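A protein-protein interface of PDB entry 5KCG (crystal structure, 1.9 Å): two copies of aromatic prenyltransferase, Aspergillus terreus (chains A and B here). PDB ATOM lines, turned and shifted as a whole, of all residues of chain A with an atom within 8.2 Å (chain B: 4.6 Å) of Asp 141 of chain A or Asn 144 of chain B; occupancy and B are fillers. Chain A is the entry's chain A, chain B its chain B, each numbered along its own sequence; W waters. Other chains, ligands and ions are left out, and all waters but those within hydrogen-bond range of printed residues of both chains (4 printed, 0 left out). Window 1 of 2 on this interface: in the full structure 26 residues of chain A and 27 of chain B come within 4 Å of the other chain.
The side-chain carboxylate of Glu 211 of chain A sits close to the backbone carbonyl oxygen of Gln 146 of chain B (3.4 Å). The side-chain carboxylate of Asp 141 of chain A lies close to the side-chain amide oxygen of Asn 144 of chain B (3.1 Å). ND1 of His 142 of chain A sits at hydrogen-bond distance from OE1 of Gln 146 of chain B (3.3 Å). OE1 of Gln 146 of chain A sits at hydrogen-bond distance from ND1 of His 142 of chain B (3.2 Å). NH1 of Arg 138 of chain A lies within hydrogen-bond range of O of Gly 148 of chain B, at 3.1 Å. The side-chain amide nitrogen (ND2) of Asn 144 of chain A lies within hydrogen-bond range of the side-chain carboxylate (OD2) of Asp 141 of chain B (3.1 Å). The guanidinium group (NH2) of Arg 122 of chain A lies within hydrogen-bond range of the side-chain amide oxygen (OD1) of Asn 144 of chain B (3.4 Å).
The guanidinium group (NH2) of Arg 138 of chain A lies within salt-bridge range of the side-chain carboxylate (OD2) of Asp 136 of chain A. OE1 of Gln 146 of chain A lies close to O of His 142 of chain A. O of His 142 of chain B sits close to OE1 of Gln 146 of chain B, at 3.2 Å. The guanidinium group (NE) of Arg 122 of chain A is in salt-bridge range of the side-chain carboxylate (OD1) of Asp 141 of chain A, at 2.8 Å.
Arg 138 of chain A touches Ala 145 of chain B (O to CB, 3.3 Å). CB of Asp 141 of chain A touches O of Asp 141 of chain B, at 3.5 Å. N of His 142 of chain A touches CB of Ala 145 of chain B, at 3.6 Å. Ala 145 of chain A touches His 142 of chain B.
Printed residues of chain B within 4 Å of Arg 122 of chain A: Asn 144 (3.4 Å). Printed residues of chain B within 4 Å of Arg 138 of chain A: Ala 145 and Gly 148. Of chain B, only Asp 141 and Asn 144 come within 4 Å of Asp 141 of chain A. Printed residues of chain B within 4 Å of Ala 145 of chain A: His 142 (3.5 Å). Printed residues of chain A within 4 Å of Asp 141 of chain B: Asp 141 (3.5 Å) and Asn 144 (3.1 Å). Printed residues of chain A within 4 Å of His 142 of chain B: Ala 145 and Gln 146. Of chain A, only Arg 122 and Asp 141 come within 4 Å of Asn 144 of chain B.
Of the 20 printed residues of chain A, 8 touch a printed residue of chain B. Along chain A the printed residues that touch a printed residue of chain B span positions 122 to 211. Hydrophobic or aromatic side chains of chain B within 4 Å of the printed part of chain A: His 142 and Ala 145. Along chain B the printed residues that touch a printed residue of chain A span positions 141 to 148. Among the printed residues, 11 pairs touch across the chains. Among the printed residues, no Asp or Glu carboxylate lies within 4 Å of a Lys or Arg side-chain nitrogen of the other chain.
Asp 141 of chain A touches its own counterpart, Asp 141 of chain B. Asp 141 of chain A touches Asn 144 of chain B, and with the chains exchanged Asn 144 of chain A touches Asp 141 of chain B. His 142 of chain A touches Ala 145 of chain B, and with the chains exchanged Ala 145 of chain A touches His 142 of chain B. His 142 of chain A touches Gln 146 of chain B, and with the chains exchanged Gln 146 of chain A touches His 142 of chain B. 10 positions are printed for both chains.
Water W2 bridges the side-chain carboxylate of Asp 141 of chain B and the backbone carbonyl oxygen of Asn 144 of chain A. Water W1 lies within hydrogen-bond range of the side-chain carboxylate (OD2) of Asp 141 of chain A (2.8 Å) and the backbone carbonyl oxygen (O) of Asn 144 of chain B (3.3 Å). Water W3 lies within hydrogen-bond range of NE2 of Gln 146 of chain B (2.8 Å), N of Glu 211 of chain A (2.9 Å) and ND1 of His 142 of chain A (3.4 Å). Water W4 bridges OD1 of Asn 144 of chain B and NH2 of Arg 122 of chain A.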
ATOM      1  N   ARG A 122      -9.007 -17.034   0.975  1.00  0.00           N
ATOM      2  CA  ARG A 122      -8.054 -16.918   2.097  1.00  0.00           C
ATOM      3  C   ARG A 122      -8.641 -16.235   3.344  1.00  0.00           C
ATOM      4  O   ARG A 122      -8.366 -16.636   4.483  1.00  0.00           O
ATOM      5  CB  ARG A 122      -6.771 -16.219   1.626  1.00  0.00           C
ATOM      6  CG  ARG A 122      -5.618 -16.063   2.609  1.00  0.00           C
ATOM      7  CD  ARG A 122      -5.274 -17.304   3.312  1.00  0.00           C
ATOM      8  NE  ARG A 122      -3.888 -17.244   3.922  1.00  0.00           N
ATOM      9  CZ  ARG A 122      -3.598 -16.718   5.127  1.00  0.00           C
ATOM     10  NH1 ARG A 122      -4.515 -16.004   5.810  1.00  0.00           N
ATOM     11  NH2 ARG A 122      -2.394 -16.871   5.637  1.00  0.00           N
ATOM     12  N   LEU A 125     -10.746 -18.774   4.942  1.00  0.00           N
ATOM     13  CA  LEU A 125      -9.901 -19.805   5.546  1.00  0.00           C
ATOM     14  C   LEU A 125      -9.242 -19.368   6.856  1.00  0.00           C
ATOM     15  O   LEU A 125      -9.130 -20.176   7.813  1.00  0.00           O
ATOM     16  CB  LEU A 125      -8.865 -20.297   4.551  1.00  0.00           C
ATOM     17  CG  LEU A 125      -9.477 -21.243   3.498  1.00  0.00           C
ATOM     18  CD1 LEU A 125      -8.495 -21.483   2.373  1.00  0.00           C
ATOM     19  CD2 LEU A 125      -9.865 -22.599   4.104  1.00  0.00           C
ATOM     20  N   ASP A 136      -5.030 -25.741   8.726  1.00  0.00           N
ATOM     21  CA  ASP A 136      -3.642 -25.385   8.548  1.00  0.00           C
ATOM     22  C   ASP A 136      -3.578 -24.746   7.215  1.00  0.00           C
ATOM     23  O   ASP A 136      -4.040 -25.328   6.240  1.00  0.00           O
ATOM     24  CB  ASP A 136      -2.822 -26.681   8.561  1.00  0.00           C
ATOM     25  CG  ASP A 136      -1.343 -26.463   8.554  1.00  0.00           C
ATOM     26  OD1 ASP A 136      -0.804 -25.540   7.887  1.00  0.00           O
ATOM     27  OD2 ASP A 136      -0.662 -27.292   9.230  1.00  0.00           O
ATOM     28  N   LEU A 137      -3.113 -23.498   7.155  1.00  0.00           N
ATOM     29  CA  LEU A 137      -3.089 -22.715   5.885  1.00  0.00           C
ATOM     30  C   LEU A 137      -1.811 -22.759   5.106  1.00  0.00           C
ATOM     31  O   LEU A 137      -1.651 -22.045   4.089  1.00  0.00           O
ATOM     32  CB  LEU A 137      -3.424 -21.267   6.178  1.00  0.00           C
ATOM     33  CG  LEU A 137      -4.797 -21.016   6.850  1.00  0.00           C
ATOM     34  CD1 LEU A 137      -5.074 -19.544   6.754  1.00  0.00           C
ATOM     35  CD2 LEU A 137      -5.922 -21.803   6.255  1.00  0.00           C
ATOM     36  N   ARG A 138      -0.871 -23.591   5.531  1.00  0.00           N
ATOM     37  CA  ARG A 138       0.444 -23.512   4.924  1.00  0.00           C
ATOM     38  C   ARG A 138       0.454 -23.997   3.493  1.00  0.00           C
ATOM     39  O   ARG A 138       1.148 -23.400   2.657  1.00  0.00           O
ATOM     40  CB  ARG A 138       1.482 -24.218   5.776  1.00  0.00           C
ATOM     41  CG  ARG A 138       1.761 -23.438   7.070  1.00  0.00           C
ATOM     42  CD  ARG A 138       2.667 -24.246   7.988  1.00  0.00           C
ATOM     43  NE  ARG A 138       2.023 -25.428   8.529  1.00  0.00           N
ATOM     44  CZ  ARG A 138       2.571 -26.140   9.521  1.00  0.00           C
ATOM     45  NH1 ARG A 138       3.751 -25.788  10.000  1.00  0.00           N
ATOM     46  NH2 ARG A 138       1.968 -27.157  10.025  1.00  0.00           N
ATOM     47  N   LEU A 139      -0.336 -25.009   3.152  1.00  0.00           N
ATOM     48  CA  LEU A 139      -0.370 -25.390   1.779  1.00  0.00           C
ATOM     49  C   LEU A 139      -1.093 -24.391   0.867  1.00  0.00           C
ATOM     50  O   LEU A 139      -0.721 -24.258  -0.329  1.00  0.00           O
ATOM     51  CB  LEU A 139      -0.928 -26.809   1.608  1.00  0.00           C
ATOM     52  CG  LEU A 139       0.063 -27.962   1.963  1.00  0.00           C
ATOM     53  CD1 LEU A 139      -0.667 -29.301   2.022  1.00  0.00           C
ATOM     54  CD2 LEU A 139       1.205 -28.043   0.955  1.00  0.00           C
ATOM     55  N   PHE A 140      -2.179 -23.823   1.374  1.00  0.00           N
ATOM     56  CA  PHE A 140      -2.854 -22.768   0.694  1.00  0.00           C
ATOM     57  C   PHE A 140      -1.824 -21.704   0.339  1.00  0.00           C
ATOM     58  O   PHE A 140      -1.717 -21.251  -0.785  1.00  0.00           O
ATOM     59  CB  PHE A 140      -3.956 -22.174   1.513  1.00  0.00           C
ATOM     60  CG  PHE A 140      -4.712 -21.108   0.762  1.00  0.00           C
ATOM     61  CD1 PHE A 140      -4.212 -19.810   0.663  1.00  0.00           C
ATOM     62  CD2 PHE A 140      -5.924 -21.393   0.171  1.00  0.00           C
ATOM     63  CE1 PHE A 140      -4.890 -18.825  -0.038  1.00  0.00           C
ATOM     64  CE2 PHE A 140      -6.621 -20.405  -0.505  1.00  0.00           C
ATOM     65  CZ  PHE A 140      -6.093 -19.139  -0.638  1.00  0.00           C
ATOM     66  N   ASP A 141      -1.083 -21.246   1.335  1.00  0.00           N
ATOM     67  CA  ASP A 141      -0.166 -20.153   1.119  1.00  0.00           C
ATOM     68  C   ASP A 141       0.903 -20.498   0.165  1.00  0.00           C
ATOM     69  O   ASP A 141       1.285 -19.690  -0.671  1.00  0.00           O
ATOM     70  CB  ASP A 141       0.412 -19.627   2.458  1.00  0.00           C
ATOM     71  CG  ASP A 141      -0.629 -18.829   3.277  1.00  0.00           C
ATOM     72  OD1 ASP A 141      -1.676 -18.366   2.708  1.00  0.00           O
ATOM     73  OD2 ASP A 141      -0.428 -18.674   4.526  1.00  0.00           O
ATOM     74  N   HIS A 142       1.417 -21.740   0.247  1.00  0.00           N
ATOM     75  CA  HIS A 142       2.407 -22.159  -0.719  1.00  0.00           C
ATOM     76  C   HIS A 142       1.928 -22.030  -2.168  1.00  0.00           C
ATOM     77  O   HIS A 142       2.663 -21.466  -3.048  1.00  0.00           O
ATOM     78  CB  HIS A 142       2.818 -23.642  -0.433  1.00  0.00           C
ATOM     79  CG  HIS A 142       3.740 -24.169  -1.439  1.00  0.00           C
ATOM     80  ND1 HIS A 142       5.076 -23.853  -1.443  1.00  0.00           N
ATOM     81  CD2 HIS A 142       3.505 -24.848  -2.601  1.00  0.00           C
ATOM     82  CE1 HIS A 142       5.636 -24.334  -2.530  1.00  0.00           C
ATOM     83  NE2 HIS A 142       4.717 -24.984  -3.231  1.00  0.00           N
ATOM     84  N   PHE A 143       0.759 -22.614  -2.465  1.00  0.00           N
ATOM     85  CA  PHE A 143       0.266 -22.604  -3.836  1.00  0.00           C
ATOM     86  C   PHE A 143      -0.243 -21.187  -4.245  1.00  0.00           C
ATOM     87  O   PHE A 143      -0.044 -20.751  -5.401  1.00  0.00           O
ATOM     88  CB  PHE A 143      -0.753 -23.672  -4.067  1.00  0.00           C
ATOM     89  CG  PHE A 143      -0.144 -25.009  -4.179  1.00  0.00           C
ATOM     90  CD1 PHE A 143       0.644 -25.274  -5.278  1.00  0.00           C
ATOM     91  CD2 PHE A 143      -0.224 -25.928  -3.186  1.00  0.00           C
ATOM     92  CE1 PHE A 143       1.341 -26.498  -5.424  1.00  0.00           C
ATOM     93  CE2 PHE A 143       0.512 -27.142  -3.278  1.00  0.00           C
ATOM     94  CZ  PHE A 143       1.242 -27.443  -4.415  1.00  0.00           C
ATOM     95  N   ASN A 144      -0.744 -20.448  -3.311  1.00  0.00           N
ATOM     96  CA  ASN A 144      -1.120 -19.068  -3.589  1.00  0.00           C
ATOM     97  C   ASN A 144       0.140 -18.274  -3.990  1.00  0.00           C
ATOM     98  O   ASN A 144       0.124 -17.454  -4.933  1.00  0.00           O
ATOM     99  CB  ASN A 144      -1.848 -18.433  -2.402  1.00  0.00           C
ATOM    100  CG  ASN A 144      -2.756 -17.236  -2.837  1.00  0.00           C
ATOM    101  OD1 ASN A 144      -3.309 -17.222  -3.965  1.00  0.00           O
ATOM    102  ND2 ASN A 144      -2.874 -16.236  -1.967  1.00  0.00           N
ATOM    103  N   ALA A 145       1.272 -18.590  -3.372  1.00  0.00           N
ATOM    104  CA  ALA A 145       2.514 -17.943  -3.737  1.00  0.00           C
ATOM    105  C   ALA A 145       3.003 -18.337  -5.125  1.00  0.00           C
ATOM    106  O   ALA A 145       3.446 -17.492  -5.881  1.00  0.00           O
ATOM    107  CB  ALA A 145       3.594 -18.216  -2.701  1.00  0.00           C
ATOM    108  N   GLN A 146       2.884 -19.602  -5.493  1.00  0.00           N
ATOM    109  CA  GLN A 146       3.499 -20.103  -6.714  1.00  0.00           C
ATOM    110  C   GLN A 146       2.608 -19.971  -7.960  1.00  0.00           C
ATOM    111  O   GLN A 146       3.124 -19.788  -9.043  1.00  0.00           O
ATOM    112  CB  GLN A 146       3.837 -21.621  -6.544  1.00  0.00           C
ATOM    113  CG  GLN A 146       4.663 -22.027  -5.326  1.00  0.00           C
ATOM    114  CD  GLN A 146       5.658 -21.025  -4.684  1.00  0.00           C
ATOM    115  OE1 GLN A 146       5.830 -20.972  -3.384  1.00  0.00           O
ATOM    116  NE2 GLN A 146       6.324 -20.248  -5.509  1.00  0.00           N
ATOM    117  N   VAL A 147       1.294 -20.106  -7.824  1.00  0.00           N
ATOM    118  CA  VAL A 147       0.431 -19.949  -8.965  1.00  0.00           C
ATOM    119  C   VAL A 147      -0.490 -18.698  -8.932  1.00  0.00           C
ATOM    120  O   VAL A 147      -1.187 -18.448  -9.920  1.00  0.00           O
ATOM    121  CB  VAL A 147      -0.391 -21.203  -9.297  1.00  0.00           C
ATOM    122  CG1 VAL A 147       0.475 -22.441  -9.274  1.00  0.00           C
ATOM    123  CG2 VAL A 147      -1.598 -21.315  -8.424  1.00  0.00           C
ATOM    124  N   GLY A 148      -0.489 -17.930  -7.831  1.00  0.00           N
ATOM    125  CA  GLY A 148      -1.196 -16.654  -7.831  1.00  0.00           C
ATOM    126  C   GLY A 148      -0.575 -15.619  -8.748  1.00  0.00           C
ATOM    127  O   GLY A 148       0.587 -15.711  -9.160  1.00  0.00           O
ATOM    128  N   VAL A 184      -8.913 -26.953  -0.978  1.00  0.00           N
ATOM    129  CA  VAL A 184      -8.944 -25.924  -2.008  1.00  0.00           C
ATOM    130  C   VAL A 184      -8.397 -26.462  -3.303  1.00  0.00           C
ATOM    131  O   VAL A 184      -7.545 -27.381  -3.316  1.00  0.00           O
ATOM    132  CB  VAL A 184      -8.155 -24.664  -1.598  1.00  0.00           C
ATOM    133  CG1 VAL A 184      -8.815 -23.988  -0.416  1.00  0.00           C
ATOM    134  CG2 VAL A 184      -6.702 -24.979  -1.284  1.00  0.00           C
ATOM    135  N   PHE A 186      -6.566 -24.825  -6.774  1.00  0.00           N
ATOM    136  CA  PHE A 186      -6.011 -23.678  -7.482  1.00  0.00           C
ATOM    137  C   PHE A 186      -5.979 -23.899  -8.968  1.00  0.00           C
ATOM    138  O   PHE A 186      -5.576 -24.971  -9.431  1.00  0.00           O
ATOM    139  CB  PHE A 186      -4.569 -23.424  -7.029  1.00  0.00           C
ATOM    140  CG  PHE A 186      -4.464 -22.891  -5.661  1.00  0.00           C
ATOM    141  CD1 PHE A 186      -4.458 -23.741  -4.566  1.00  0.00           C
ATOM    142  CD2 PHE A 186      -4.382 -21.507  -5.462  1.00  0.00           C
ATOM    143  CE1 PHE A 186      -4.312 -23.191  -3.284  1.00  0.00           C
ATOM    144  CE2 PHE A 186      -4.239 -20.983  -4.180  1.00  0.00           C
ATOM    145  CZ  PHE A 186      -4.260 -21.814  -3.116  1.00  0.00           C
ATOM    146  N   GLU A 211       7.808 -27.826   0.715  1.00  0.00           N
ATOM    147  CA  GLU A 211       8.661 -28.411   1.790  1.00  0.00           C
ATOM    148  C   GLU A 211       8.487 -29.937   1.943  1.00  0.00           C
ATOM    149  O   GLU A 211       9.467 -30.675   2.027  1.00  0.00           O
ATOM    150  CB  GLU A 211       8.343 -27.725   3.127  1.00  0.00           C
ATOM    151  CG  GLU A 211       9.361 -27.986   4.211  1.00  0.00           C
ATOM    152  CD  GLU A 211       8.986 -27.237   5.493  1.00  0.00           C
ATOM    153  OE1 GLU A 211       8.870 -27.890   6.514  1.00  0.00           O
ATOM    154  OE2 GLU A 211       8.782 -25.996   5.470  1.00  0.00           O
ATOM    155  N   VAL A 250      -5.297 -29.171  -2.626  1.00  0.00           N
ATOM    156  CA  VAL A 250      -4.782 -29.591  -1.335  1.00  0.00           C
ATOM    157  C   VAL A 250      -5.845 -29.600  -0.296  1.00  0.00           C
ATOM    158  O   VAL A 250      -6.848 -28.895  -0.399  1.00  0.00           O
ATOM    159  CB  VAL A 250      -3.578 -28.737  -0.859  1.00  0.00           C
ATOM    160  CG1 VAL A 250      -2.336 -28.952  -1.758  1.00  0.00           C
ATOM    161  CG2 VAL A 250      -3.920 -27.249  -0.816  1.00  0.00           C
ATOM    162  N   CYS A 252      -6.478 -28.429   3.573  1.00  0.00           N
ATOM    163  CA  CYS A 252      -5.938 -27.341   4.432  1.00  0.00           C
ATOM    164  C   CYS A 252      -5.788 -27.906   5.851  1.00  0.00           C
ATOM    165  O   CYS A 252      -6.481 -27.480   6.807  1.00  0.00           O
ATOM    166  CB  CYS A 252      -6.853 -26.110   4.490  1.00  0.00           C
ATOM    167  SG  CYS A 252      -6.892 -25.356   2.836  1.00  0.00           S
ATOM    168  N   PHE B 140       5.195 -12.891   0.820  1.00  0.00           N
ATOM    169  CA  PHE B 140       4.618 -13.101   2.118  1.00  0.00           C
ATOM    170  C   PHE B 140       4.125 -14.531   2.230  1.00  0.00           C
ATOM    171  O   PHE B 140       4.403 -15.201   3.193  1.00  0.00           O
ATOM    172  CB  PHE B 140       3.426 -12.103   2.405  1.00  0.00           C
ATOM    173  CG  PHE B 140       2.863 -12.244   3.800  1.00  0.00           C
ATOM    174  CD1 PHE B 140       1.993 -13.234   4.115  1.00  0.00           C
ATOM    175  CD2 PHE B 140       3.231 -11.362   4.831  1.00  0.00           C
ATOM    176  CE1 PHE B 140       1.518 -13.417   5.429  1.00  0.00           C
ATOM    177  CE2 PHE B 140       2.774 -11.523   6.123  1.00  0.00           C
ATOM    178  CZ  PHE B 140       1.899 -12.543   6.428  1.00  0.00           C
ATOM    179  N   ASP B 141       3.302 -14.940   1.298  1.00  0.00           N
ATOM    180  CA  ASP B 141       2.669 -16.214   1.365  1.00  0.00           C
ATOM    181  C   ASP B 141       3.712 -17.298   1.294  1.00  0.00           C
ATOM    182  O   ASP B 141       3.588 -18.287   1.989  1.00  0.00           O
ATOM    183  CB  ASP B 141       1.636 -16.364   0.294  1.00  0.00           C
ATOM    184  CG  ASP B 141       0.327 -15.522   0.597  1.00  0.00           C
ATOM    185  OD1 ASP B 141       0.111 -15.122   1.770  1.00  0.00           O
ATOM    186  OD2 ASP B 141      -0.459 -15.270  -0.342  1.00  0.00           O
ATOM    187  N   HIS B 142       4.719 -17.093   0.472  1.00  0.00           N
ATOM    188  CA  HIS B 142       5.796 -18.075   0.428  1.00  0.00           C
ATOM    189  C   HIS B 142       6.466 -18.334   1.768  1.00  0.00           C
ATOM    190  O   HIS B 142       6.589 -19.492   2.239  1.00  0.00           O
ATOM    191  CB  HIS B 142       6.839 -17.657  -0.606  1.00  0.00           C
ATOM    192  CG  HIS B 142       7.997 -18.588  -0.630  1.00  0.00           C
ATOM    193  ND1 HIS B 142       7.933 -19.811  -1.245  1.00  0.00           N
ATOM    194  CD2 HIS B 142       9.201 -18.527   0.001  1.00  0.00           C
ATOM    195  CE1 HIS B 142       9.071 -20.461  -1.039  1.00  0.00           C
ATOM    196  NE2 HIS B 142       9.833 -19.729  -0.250  1.00  0.00           N
ATOM    197  N   PHE B 143       6.911 -17.259   2.431  1.00  0.00           N
ATOM    198  CA  PHE B 143       7.568 -17.434   3.741  1.00  0.00           C
ATOM    199  C   PHE B 143       6.610 -17.817   4.863  1.00  0.00           C
ATOM    200  O   PHE B 143       6.944 -18.610   5.769  1.00  0.00           O
ATOM    201  CB  PHE B 143       8.428 -16.219   4.016  1.00  0.00           C
ATOM    202  CG  PHE B 143       9.667 -16.211   3.176  1.00  0.00           C
ATOM    203  CD1 PHE B 143      10.673 -17.152   3.452  1.00  0.00           C
ATOM    204  CD2 PHE B 143       9.846 -15.338   2.137  1.00  0.00           C
ATOM    205  CE1 PHE B 143      11.834 -17.207   2.669  1.00  0.00           C
ATOM    206  CE2 PHE B 143      10.992 -15.389   1.346  1.00  0.00           C
ATOM    207  CZ  PHE B 143      12.003 -16.325   1.627  1.00  0.00           C
ATOM    208  N   ASN B 144       5.366 -17.362   4.803  1.00  0.00           N
ATOM    209  CA  ASN B 144       4.405 -17.777   5.787  1.00  0.00           C
ATOM    210  C   ASN B 144       4.245 -19.344   5.661  1.00  0.00           C
ATOM    211  O   ASN B 144       4.000 -20.023   6.636  1.00  0.00           O
ATOM    212  CB  ASN B 144       3.089 -16.995   5.557  1.00  0.00           C
ATOM    213  CG  ASN B 144       2.140 -16.976   6.771  1.00  0.00           C
ATOM    214  OD1 ASN B 144       0.898 -16.836   6.617  1.00  0.00           O
ATOM    215  ND2 ASN B 144       2.689 -17.062   7.951  1.00  0.00           N
ATOM    216  N   ALA B 145       4.255 -19.844   4.463  1.00  0.00           N
ATOM    217  CA  ALA B 145       4.084 -21.267   4.257  1.00  0.00           C
ATOM    218  C   ALA B 145       5.276 -22.032   4.838  1.00  0.00           C
ATOM    219  O   ALA B 145       5.091 -23.068   5.408  1.00  0.00           O
ATOM    220  CB  ALA B 145       3.951 -21.576   2.786  1.00  0.00           C
ATOM    221  N   GLN B 146       6.480 -21.509   4.663  1.00  0.00           N
ATOM    222  CA  GLN B 146       7.717 -22.253   4.941  1.00  0.00           C
ATOM    223  C   GLN B 146       8.153 -22.043   6.376  1.00  0.00           C
ATOM    224  O   GLN B 146       8.716 -22.966   6.960  1.00  0.00           O
ATOM    225  CB  GLN B 146       8.871 -21.796   4.014  1.00  0.00           C
ATOM    226  CG  GLN B 146       8.660 -21.766   2.512  1.00  0.00           C
ATOM    227  CD  GLN B 146       7.663 -22.728   1.868  1.00  0.00           C
ATOM    228  OE1 GLN B 146       6.933 -22.370   0.865  1.00  0.00           O
ATOM    229  NE2 GLN B 146       7.631 -23.954   2.373  1.00  0.00           N
ATOM    230  N   VAL B 147       7.854 -20.880   6.996  1.00  0.00           N
ATOM    231  CA  VAL B 147       8.183 -20.702   8.418  1.00  0.00           C
ATOM    232  C   VAL B 147       7.064 -20.547   9.394  1.00  0.00           C
ATOM    233  O   VAL B 147       7.310 -20.507  10.613  1.00  0.00           O
ATOM    234  CB  VAL B 147       9.262 -19.630   8.621  1.00  0.00           C
ATOM    235  CG1 VAL B 147      10.374 -19.824   7.604  1.00  0.00           C
ATOM    236  CG2 VAL B 147       8.713 -18.258   8.484  1.00  0.00           C
ATOM    237  N   GLY B 148       5.806 -20.516   8.933  1.00  0.00           N
ATOM    238  CA  GLY B 148       4.716 -20.486   9.850  1.00  0.00           C
ATOM    239  C   GLY B 148       4.440 -21.821  10.564  1.00  0.00           C
ATOM    240  O   GLY B 148       4.930 -22.879  10.198  1.00  0.00           O
ATOM    241  N   PHE B 186       9.877 -12.191   8.880  1.00  0.00           N
ATOM    242  CA  PHE B 186       9.447 -13.416   9.490  1.00  0.00           C
ATOM    243  C   PHE B 186      10.484 -13.870  10.468  1.00  0.00           C
ATOM    244  O   PHE B 186      11.669 -13.948  10.125  1.00  0.00           O
ATOM    245  CB  PHE B 186       9.235 -14.508   8.447  1.00  0.00           C
ATOM    246  CG  PHE B 186       7.985 -14.302   7.592  1.00  0.00           C
ATOM    247  CD1 PHE B 186       6.751 -14.819   7.998  1.00  0.00           C
ATOM    248  CD2 PHE B 186       8.059 -13.598   6.414  1.00  0.00           C
ATOM    249  CE1 PHE B 186       5.628 -14.574   7.232  1.00  0.00           C
ATOM    250  CE2 PHE B 186       6.930 -13.396   5.653  1.00  0.00           C
ATOM    251  CZ  PHE B 186       5.747 -13.858   6.068  1.00  0.00           C
HETATM  252  O   HOH W   1       0.783 -20.399   6.296  1.00  0.00           O
HETATM  253  O   HOH W   2       0.201 -14.852  -2.915  1.00  0.00           O
HETATM  254  O   HOH W   3       5.823 -25.741   1.254  1.00  0.00           O
HETATM  255  O   HOH W   4      -1.452 -16.977   8.569  1.00  0.00           O
